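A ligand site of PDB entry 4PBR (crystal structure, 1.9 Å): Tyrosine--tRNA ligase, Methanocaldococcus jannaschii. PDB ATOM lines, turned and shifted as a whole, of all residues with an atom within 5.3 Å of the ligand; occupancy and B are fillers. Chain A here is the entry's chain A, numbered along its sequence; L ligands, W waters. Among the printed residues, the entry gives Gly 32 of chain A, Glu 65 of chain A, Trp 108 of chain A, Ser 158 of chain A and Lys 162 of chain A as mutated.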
ATOM      1  N   GLY A  32      10.902  14.212  18.407  1.00  0.00           N
ATOM      2  CA  GLY A  32       9.533  13.766  18.514  1.00  0.00           C
ATOM      3  C   GLY A  32       8.619  14.398  17.490  1.00  0.00           C
ATOM      4  O   GLY A  32       8.855  15.508  17.013  1.00  0.00           O
ATOM      5  N   ILE A  33       7.568  13.662  17.169  1.00  0.00           N
ATOM      6  CA  ILE A  33       6.412  14.201  16.473  1.00  0.00           C
ATOM      7  C   ILE A  33       5.192  13.433  16.971  1.00  0.00           C
ATOM      8  O   ILE A  33       5.317  12.315  17.458  1.00  0.00           O
ATOM      9  CB  ILE A  33       6.590  14.102  14.931  1.00  0.00           C
ATOM     10  CG1 ILE A  33       5.380  14.640  14.186  1.00  0.00           C
ATOM     11  CG2 ILE A  33       6.884  12.666  14.499  1.00  0.00           C
ATOM     12  CD1 ILE A  33       5.672  14.758  12.667  1.00  0.00           C
ATOM     13  N   GLY A  34       4.028  14.042  16.868  1.00  0.00           N
ATOM     14  CA  GLY A  34       2.789  13.383  17.232  1.00  0.00           C
ATOM     15  C   GLY A  34       1.783  13.471  16.118  1.00  0.00           C
ATOM     16  O   GLY A  34       1.736  14.459  15.369  1.00  0.00           O
ATOM     17  N   PHE A  35       0.985  12.419  15.991  1.00  0.00           N
ATOM     18  CA  PHE A  35      -0.088  12.381  15.012  1.00  0.00           C
ATOM     19  C   PHE A  35      -1.389  12.027  15.711  1.00  0.00           C
ATOM     20  O   PHE A  35      -1.480  10.975  16.344  1.00  0.00           O
ATOM     21  CB  PHE A  35       0.156  11.360  13.896  1.00  0.00           C
ATOM     22  CG  PHE A  35       1.481  11.500  13.198  1.00  0.00           C
ATOM     23  CD1 PHE A  35       1.625  12.368  12.121  1.00  0.00           C
ATOM     24  CD2 PHE A  35       2.569  10.749  13.602  1.00  0.00           C
ATOM     25  CE1 PHE A  35       2.843  12.483  11.452  1.00  0.00           C
ATOM     26  CE2 PHE A  35       3.792  10.858  12.949  1.00  0.00           C
ATOM     27  CZ  PHE A  35       3.927  11.730  11.870  1.00  0.00           C
ATOM     28  N   GLU A  36      -2.386  12.899  15.588  1.00  0.00           N
ATOM     29  CA  GLU A  36      -3.756  12.468  15.794  1.00  0.00           C
ATOM     30  C   GLU A  36      -4.030  11.263  14.906  1.00  0.00           C
ATOM     31  O   GLU A  36      -3.788  11.331  13.688  1.00  0.00           O
ATOM     32  CB  GLU A  36      -4.723  13.591  15.451  1.00  0.00           C
ATOM     33  CG  GLU A  36      -4.659  14.757  16.435  1.00  0.00           C
ATOM     34  CD  GLU A  36      -5.781  15.725  16.222  1.00  0.00           C
ATOM     35  OE1 GLU A  36      -6.889  15.261  15.896  1.00  0.00           O
ATOM     36  OE2 GLU A  36      -5.544  16.954  16.377  1.00  0.00           O
ATOM     37  N   ILE A  63      10.755   9.537  18.948  1.00  0.00           N
ATOM     38  CA  ILE A  63       9.542   9.288  19.721  1.00  0.00           C
ATOM     39  C   ILE A  63       8.366   9.684  18.855  1.00  0.00           C
ATOM     40  O   ILE A  63       8.303  10.808  18.353  1.00  0.00           O
ATOM     41  CB  ILE A  63       9.532  10.072  21.051  1.00  0.00           C
ATOM     42  CG1 ILE A  63      10.851   9.839  21.806  1.00  0.00           C
ATOM     43  CG2 ILE A  63       8.352   9.661  21.912  1.00  0.00           C
ATOM     44  CD1 ILE A  63      10.949  10.539  23.146  1.00  0.00           C
ATOM     45  N   ILE A  64       7.446   8.741  18.641  1.00  0.00           N
ATOM     46  CA  ILE A  64       6.226   8.989  17.876  1.00  0.00           C
ATOM     47  C   ILE A  64       5.059   8.943  18.851  1.00  0.00           C
ATOM     48  O   ILE A  64       4.750   7.880  19.416  1.00  0.00           O
ATOM     49  CB  ILE A  64       6.005   7.970  16.753  1.00  0.00           C
ATOM     50  CG1 ILE A  64       7.253   7.856  15.852  1.00  0.00           C
ATOM     51  CG2 ILE A  64       4.761   8.357  15.953  1.00  0.00           C
ATOM     52  CD1 ILE A  64       7.601   9.139  15.149  1.00  0.00           C
ATOM     53  N   GLU A  65       4.407  10.078  19.061  1.00  0.00           N
ATOM     54  CA  GLU A  65       3.200  10.093  19.872  1.00  0.00           C
ATOM     55  C   GLU A  65       2.000   9.782  18.993  1.00  0.00           C
ATOM     56  O   GLU A  65       1.678  10.556  18.085  1.00  0.00           O
ATOM     57  CB  GLU A  65       3.009  11.433  20.590  1.00  0.00           C
ATOM     58  CG  GLU A  65       1.721  11.419  21.408  1.00  0.00           C
ATOM     59  CD  GLU A  65       1.472  12.698  22.203  1.00  0.00           C
ATOM     60  OE1 GLU A  65       0.287  12.930  22.539  1.00  0.00           O
ATOM     61  OE2 GLU A  65       2.434  13.434  22.486  1.00  0.00           O
ATOM     62  N   ALA A  67      -1.330  10.374  19.228  1.00  0.00           N
ATOM     63  CA  ALA A  67      -1.891  11.425  20.090  1.00  0.00           C
ATOM     64  C   ALA A  67      -3.388  11.185  20.309  1.00  0.00           C
ATOM     65  O   ALA A  67      -4.256  11.899  19.787  1.00  0.00           O
ATOM     66  CB  ALA A  67      -1.625  12.794  19.484  1.00  0.00           C
ATOM     67  N   HIS A  70      -5.165  14.020  22.202  1.00  0.00           N
ATOM     68  CA  HIS A  70      -5.285  15.163  21.299  1.00  0.00           C
ATOM     69  C   HIS A  70      -6.410  14.961  20.310  1.00  0.00           C
ATOM     70  O   HIS A  70      -7.236  15.855  20.089  1.00  0.00           O
ATOM     71  CB  HIS A  70      -3.965  15.410  20.576  1.00  0.00           C
ATOM     72  CG  HIS A  70      -2.961  16.142  21.408  1.00  0.00           C
ATOM     73  ND1 HIS A  70      -2.980  17.516  21.571  1.00  0.00           N
ATOM     74  CD2 HIS A  70      -1.904  15.700  22.122  1.00  0.00           C
ATOM     75  CE1 HIS A  70      -1.977  17.873  22.344  1.00  0.00           C
ATOM     76  NE2 HIS A  70      -1.305  16.798  22.699  1.00  0.00           N
ATOM     77  N   TRP A 108       0.929   9.159  29.545  1.00  0.00           N
ATOM     78  CA  TRP A 108       1.478  10.094  30.535  1.00  0.00           C
ATOM     79  C   TRP A 108       0.592  11.305  30.811  1.00  0.00           C
ATOM     80  O   TRP A 108       0.782  11.940  31.857  1.00  0.00           O
ATOM     81  CB  TRP A 108       2.866  10.595  30.088  1.00  0.00           C
ATOM     82  CG  TRP A 108       2.840  11.499  28.876  1.00  0.00           C
ATOM     83  CD1 TRP A 108       2.549  12.841  28.852  1.00  0.00           C
ATOM     84  CD2 TRP A 108       3.127  11.136  27.517  1.00  0.00           C
ATOM     85  NE1 TRP A 108       2.635  13.324  27.554  1.00  0.00           N
ATOM     86  CE2 TRP A 108       2.985  12.297  26.721  1.00  0.00           C
ATOM     87  CE3 TRP A 108       3.487   9.923  26.896  1.00  0.00           C
ATOM     88  CZ2 TRP A 108       3.188  12.295  25.344  1.00  0.00           C
ATOM     89  CZ3 TRP A 108       3.677   9.917  25.522  1.00  0.00           C
ATOM     90  CH2 TRP A 108       3.543  11.097  24.762  1.00  0.00           C
ATOM     91  N   ILE A 137      -5.383  23.639  12.913  1.00  0.00           N
ATOM     92  CA  ILE A 137      -5.425  22.303  13.486  1.00  0.00           C
ATOM     93  C   ILE A 137      -6.828  21.941  13.947  1.00  0.00           C
ATOM     94  O   ILE A 137      -7.289  20.826  13.723  1.00  0.00           O
ATOM     95  CB  ILE A 137      -4.423  22.188  14.655  1.00  0.00           C
ATOM     96  CG1 ILE A 137      -3.002  22.484  14.154  1.00  0.00           C
ATOM     97  CG2 ILE A 137      -4.528  20.829  15.340  1.00  0.00           C
ATOM     98  CD1 ILE A 137      -1.972  22.781  15.259  1.00  0.00           C
ATOM     99  N   TYR A 151      -5.903  21.813  24.100  1.00  0.00           N
ATOM    100  CA  TYR A 151      -5.086  21.083  23.142  1.00  0.00           C
ATOM    101  C   TYR A 151      -3.674  21.661  23.030  1.00  0.00           C
ATOM    102  O   TYR A 151      -2.697  20.928  23.264  1.00  0.00           O
ATOM    103  CB  TYR A 151      -5.862  21.069  21.822  1.00  0.00           C
ATOM    104  CG  TYR A 151      -5.254  20.258  20.700  1.00  0.00           C
ATOM    105  CD1 TYR A 151      -4.034  20.626  20.148  1.00  0.00           C
ATOM    106  CD2 TYR A 151      -5.916  19.171  20.164  1.00  0.00           C
ATOM    107  CE1 TYR A 151      -3.476  19.900  19.088  1.00  0.00           C
ATOM    108  CE2 TYR A 151      -5.376  18.439  19.119  1.00  0.00           C
ATOM    109  CZ  TYR A 151      -4.156  18.819  18.584  1.00  0.00           C
ATOM    110  OH  TYR A 151      -3.612  18.100  17.543  1.00  0.00           O
ATOM    111  N   GLN A 155       0.079  19.863  24.109  1.00  0.00           N
ATOM    112  CA  GLN A 155       1.204  19.564  23.224  1.00  0.00           C
ATOM    113  C   GLN A 155       2.497  20.172  23.768  1.00  0.00           C
ATOM    114  O   GLN A 155       3.532  19.500  23.804  1.00  0.00           O
ATOM    115  CB  GLN A 155       0.893  20.055  21.807  1.00  0.00           C
ATOM    116  CG  GLN A 155       1.974  19.773  20.788  1.00  0.00           C
ATOM    117  CD  GLN A 155       1.425  19.858  19.356  1.00  0.00           C
ATOM    118  OE1 GLN A 155       0.229  19.671  19.143  1.00  0.00           O
ATOM    119  NE2 GLN A 155       2.298  20.146  18.382  1.00  0.00           N
ATOM    120  N   SER A 158       3.712  18.144  26.731  1.00  0.00           N
ATOM    121  CA  SER A 158       4.317  16.882  26.353  1.00  0.00           C
ATOM    122  C   SER A 158       5.721  17.085  25.819  1.00  0.00           C
ATOM    123  O   SER A 158       6.623  16.281  26.100  1.00  0.00           O
ATOM    124  CB  SER A 158       3.439  16.175  25.312  1.00  0.00           C
ATOM    125  OG  SER A 158       2.265  15.661  25.928  1.00  0.00           O
ATOM    126  N   ILE A 159       5.937  18.159  25.051  1.00  0.00           N
ATOM    127  CA  ILE A 159       7.300  18.489  24.647  1.00  0.00           C
ATOM    128  C   ILE A 159       8.183  18.626  25.885  1.00  0.00           C
ATOM    129  O   ILE A 159       9.280  18.066  25.941  1.00  0.00           O
ATOM    130  CB  ILE A 159       7.304  19.784  23.799  1.00  0.00           C
ATOM    131  CG1 ILE A 159       6.763  19.497  22.402  1.00  0.00           C
ATOM    132  CG2 ILE A 159       8.703  20.328  23.686  1.00  0.00           C
ATOM    133  CD1 ILE A 159       6.504  20.746  21.594  1.00  0.00           C
ATOM    134  N   LYS A 162       8.200  14.830  27.789  1.00  0.00           N
ATOM    135  CA  LYS A 162       8.987  13.800  27.097  1.00  0.00           C
ATOM    136  C   LYS A 162      10.424  14.241  26.824  1.00  0.00           C
ATOM    137  O   LYS A 162      11.231  13.397  26.405  1.00  0.00           O
ATOM    138  CB  LYS A 162       8.309  13.380  25.801  1.00  0.00           C
ATOM    139  CG  LYS A 162       6.882  12.885  26.002  1.00  0.00           C
ATOM    140  CD  LYS A 162       6.776  11.799  27.070  1.00  0.00           C
ATOM    141  CE  LYS A 162       7.316  10.463  26.584  1.00  0.00           C
ATOM    142  NZ  LYS A 162       7.054   9.379  27.576  1.00  0.00           N
ATOM    143  N   VAL A 164      12.173  16.052  24.613  1.00  0.00           N
ATOM    144  CA  VAL A 164      12.838  15.983  23.324  1.00  0.00           C
ATOM    145  C   VAL A 164      13.716  17.208  23.103  1.00  0.00           C
ATOM    146  O   VAL A 164      13.394  18.325  23.535  1.00  0.00           O
ATOM    147  CB  VAL A 164      11.820  15.823  22.174  1.00  0.00           C
ATOM    148  CG1 VAL A 164      11.122  14.491  22.277  1.00  0.00           C
ATOM    149  CG2 VAL A 164      10.811  16.951  22.178  1.00  0.00           C
ATOM    150  N   ALA A 167      11.502  18.996  18.148  1.00  0.00           N
ATOM    151  CA  ALA A 167      10.134  18.707  17.772  1.00  0.00           C
ATOM    152  C   ALA A 167       9.978  18.892  16.276  1.00  0.00           C
ATOM    153  O   ALA A 167      10.476  19.863  15.703  1.00  0.00           O
ATOM    154  CB  ALA A 167       9.128  19.615  18.509  1.00  0.00           C
ATOM    155  N   VAL A 168       9.279  17.948  15.641  1.00  0.00           N
ATOM    156  CA  VAL A 168       9.053  17.967  14.196  1.00  0.00           C
ATOM    157  C   VAL A 168       7.551  17.990  13.945  1.00  0.00           C
ATOM    158  O   VAL A 168       6.777  17.338  14.647  1.00  0.00           O
ATOM    159  CB  VAL A 168       9.709  16.750  13.509  1.00  0.00           C
ATOM    160  CG1 VAL A 168       9.643  16.895  11.956  1.00  0.00           C
ATOM    161  CG2 VAL A 168      11.135  16.595  13.959  1.00  0.00           C
ATOM    162  N   GLU A 172       1.887  23.902  10.044  1.00  0.00           N
ATOM    163  CA  GLU A 172       0.712  24.281  10.825  1.00  0.00           C
ATOM    164  C   GLU A 172       0.943  24.148  12.324  1.00  0.00           C
ATOM    165  O   GLU A 172       0.152  24.676  13.104  1.00  0.00           O
ATOM    166  CB  GLU A 172      -0.507  23.443  10.403  1.00  0.00           C
ATOM    167  CG  GLU A 172      -0.536  22.034  10.941  1.00  0.00           C
ATOM    168  CD  GLU A 172       0.394  21.093  10.190  1.00  0.00           C
ATOM    169  OE1 GLU A 172       0.614  19.960  10.677  1.00  0.00           O
ATOM    170  OE2 GLU A 172       0.887  21.501   9.117  1.00  0.00           O
ATOM    171  N   GLN A 173       2.022  23.467  12.742  1.00  0.00           N
ATOM    172  CA  GLN A 173       2.388  23.297  14.146  1.00  0.00           C
ATOM    173  C   GLN A 173       3.273  24.434  14.675  1.00  0.00           C
ATOM    174  O   GLN A 173       3.675  24.374  15.835  1.00  0.00           O
ATOM    175  CB  GLN A 173       3.126  21.971  14.346  1.00  0.00           C
ATOM    176  CG  GLN A 173       2.439  20.729  13.757  1.00  0.00           C
ATOM    177  CD  GLN A 173       1.084  20.453  14.366  1.00  0.00           C
ATOM    178  OE1 GLN A 173       0.917  20.514  15.582  1.00  0.00           O
ATOM    179  NE2 GLN A 173       0.116  20.139  13.528  1.00  0.00           N
ATOM    180  N   ILE A 176       2.046  26.613  17.932  1.00  0.00           N
ATOM    181  CA  ILE A 176       2.152  25.791  19.137  1.00  0.00           C
ATOM    182  C   ILE A 176       3.623  25.663  19.544  1.00  0.00           C
ATOM    183  O   ILE A 176       3.982  25.842  20.722  1.00  0.00           O
ATOM    184  CB  ILE A 176       1.505  24.414  18.920  1.00  0.00           C
ATOM    185  CG1 ILE A 176      -0.016  24.522  18.816  1.00  0.00           C
ATOM    186  CG2 ILE A 176       1.876  23.471  20.041  1.00  0.00           C
ATOM    187  CD1 ILE A 176      -0.736  23.146  18.816  1.00  0.00           C
ATOM    188  N   HIS A 177       4.493  25.411  18.564  1.00  0.00           N
ATOM    189  CA  HIS A 177       5.924  25.301  18.825  1.00  0.00           C
ATOM    190  C   HIS A 177       6.507  26.614  19.328  1.00  0.00           C
ATOM    191  O   HIS A 177       7.398  26.617  20.196  1.00  0.00           O
ATOM    192  CB  HIS A 177       6.650  24.841  17.549  1.00  0.00           C
ATOM    193  CG  HIS A 177       6.488  23.379  17.275  1.00  0.00           C
ATOM    194  ND1 HIS A 177       6.848  22.808  16.071  1.00  0.00           N
ATOM    195  CD2 HIS A 177       6.007  22.369  18.044  1.00  0.00           C
ATOM    196  CE1 HIS A 177       6.584  21.509  16.107  1.00  0.00           C
ATOM    197  NE2 HIS A 177       6.072  21.217  17.294  1.00  0.00           N
HETATM  198  N1  LIG L   1      -0.947  18.953  16.749  1.00  0.00           N
HETATM  199  C1  LIG L   1      -0.725  17.746  16.074  1.00  0.00           C
HETATM  200  C2  LIG L   1      -0.745  16.619  16.978  1.00  0.00           C
HETATM  201  C3  LIG L   1       0.367  16.375  17.933  1.00  0.00           C
HETATM  202  C4  LIG L   1       0.049  15.807  19.261  1.00  0.00           C
HETATM  203  C5  LIG L   1       1.130  15.524  20.231  1.00  0.00           C
HETATM  204  C6  LIG L   1       2.528  15.886  19.866  1.00  0.00           C
HETATM  205  N2  LIG L   1       3.606  15.500  20.700  1.00  0.00           N
HETATM  206  C7  LIG L   1       4.990  15.820  20.521  1.00  0.00           C
HETATM  207  C8  LIG L   1       5.923  15.086  21.410  1.00  0.00           C
HETATM  208  C9  LIG L   1       7.230  15.800  21.506  1.00  0.00           C
HETATM  209 BR1  LIG L   1       6.249  13.422  20.431  1.00  0.00          BR
HETATM  210  C10 LIG L   1       5.335  14.725  22.727  1.00  0.00           C
HETATM  211  O1  LIG L   1       5.401  16.610  19.683  1.00  0.00           O
HETATM  212  C11 LIG L   1       2.846  16.407  18.509  1.00  0.00           C
HETATM  213  C12 LIG L   1       1.761  16.677  17.536  1.00  0.00           C
HETATM  214  C13 LIG L   1      -1.545  17.552  14.889  1.00  0.00           C
HETATM  215  O2  LIG L   1      -1.634  16.428  14.323  1.00  0.00           O
HETATM  216  O3  LIG L   1      -2.184  18.520  14.426  1.00  0.00           O
HETATM  217  O   HOH W   1       1.196  16.046  23.230  1.00  0.00           O
HETATM  218  O   HOH W   2       4.802  18.997  18.227  1.00  0.00           O
HETATM  219  O   HOH W   3       4.529  17.374  16.087  1.00  0.00           O
HETATM  220  O   HOH W   4       2.383  17.150  14.386  1.00  0.00           O
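A nitrogen (N1) of the ligand is in hydrogen-bond range of the side-chain amide oxygen (OE1) of Gln 155, at 2.8 Å.
The side-chain amide oxygen of Gln 173 lies within hydrogen-bond range of a nitrogen (N1) of the ligand (2.7 Å).
OH of Tyr 151 sits at hydrogen-bond distance from N1 of the ligand, at 2.9 Å.
OE2 of Glu 65 lies within hydrogen-bond range of N2 of the ligand (3.0 Å).
Water W2 lies within hydrogen-bond range of NE2 of His 177, NE2 of Gln 155 and O1 of the ligand.
Water W1 lies within hydrogen-bond range of NE2 of His 70, OG of Ser 158 and OE2 of Glu 65.
Water W3 bridges the backbone carbonyl oxygen (O) of Val 168 (2.7 Å) and the backbone NH (N) of Gly 34 (3.5 Å).
The side-chain carboxylate of Glu 172 sits at hydrogen-bond distance from the side-chain amide nitrogen of Gln 173.
O of Glu 65 lies within hydrogen-bond range of N of Phe 35.
The backbone NH (N) of Glu 65 sits at hydrogen-bond distance from the backbone carbonyl oxygen (O) of Ile 33, at 2.9 Å.
The side-chain amide nitrogen of Gln 155 lies within hydrogen-bond range of the side-chain amide oxygen of Gln 173, at 3.1 Å.
The backbone NH (N) of Ile 33 sits at hydrogen-bond distance from the backbone carbonyl oxygen (O) of Ile 63.
The indole nitrogen (NE1) of Trp 108 sits at hydrogen-bond distance from the side-chain hydroxyl (OG) of Ser 158 (2.9 Å).
The backbone carbonyl oxygen (O) of Phe 35 is in hydrogen-bond range of the backbone NH (N) of Ala 67 (2.9 Å).
The backbone carbonyl oxygen (O) of Gly 32 is in hydrogen-bond range of the backbone NH (N) of Val 168 (2.8 Å).
Merely in contact with the ligand: Gly 32 (3.8 Å), Ile 33 (3.3 Å), Gly 34 (3.1 Å), Glu 36 (3.8 Å), Ile 63 (3.9 Å), Ala 67 (3.5 Å), His 70 (3.5 Å), Ile 137 (3.4 Å), Ser 158 (3.5 Å), Ile 159 (3.8 Å) and Val 164 (3.8 Å).
Hydrophobic or aromatic side chains within 4 Å of the ligand: Ala 67, His 70, Ile 137, Tyr 151, Ile 159 and Val 164.
Within 4 Å of the ligand: Gly 32, Ile 33, Gly 34, Glu 36, Ile 63, Glu 65, Ala 67, His 70, Ile 137, Tyr 151, Gln 155, Ser 158, Ile 159, Val 164 and Gln 173.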
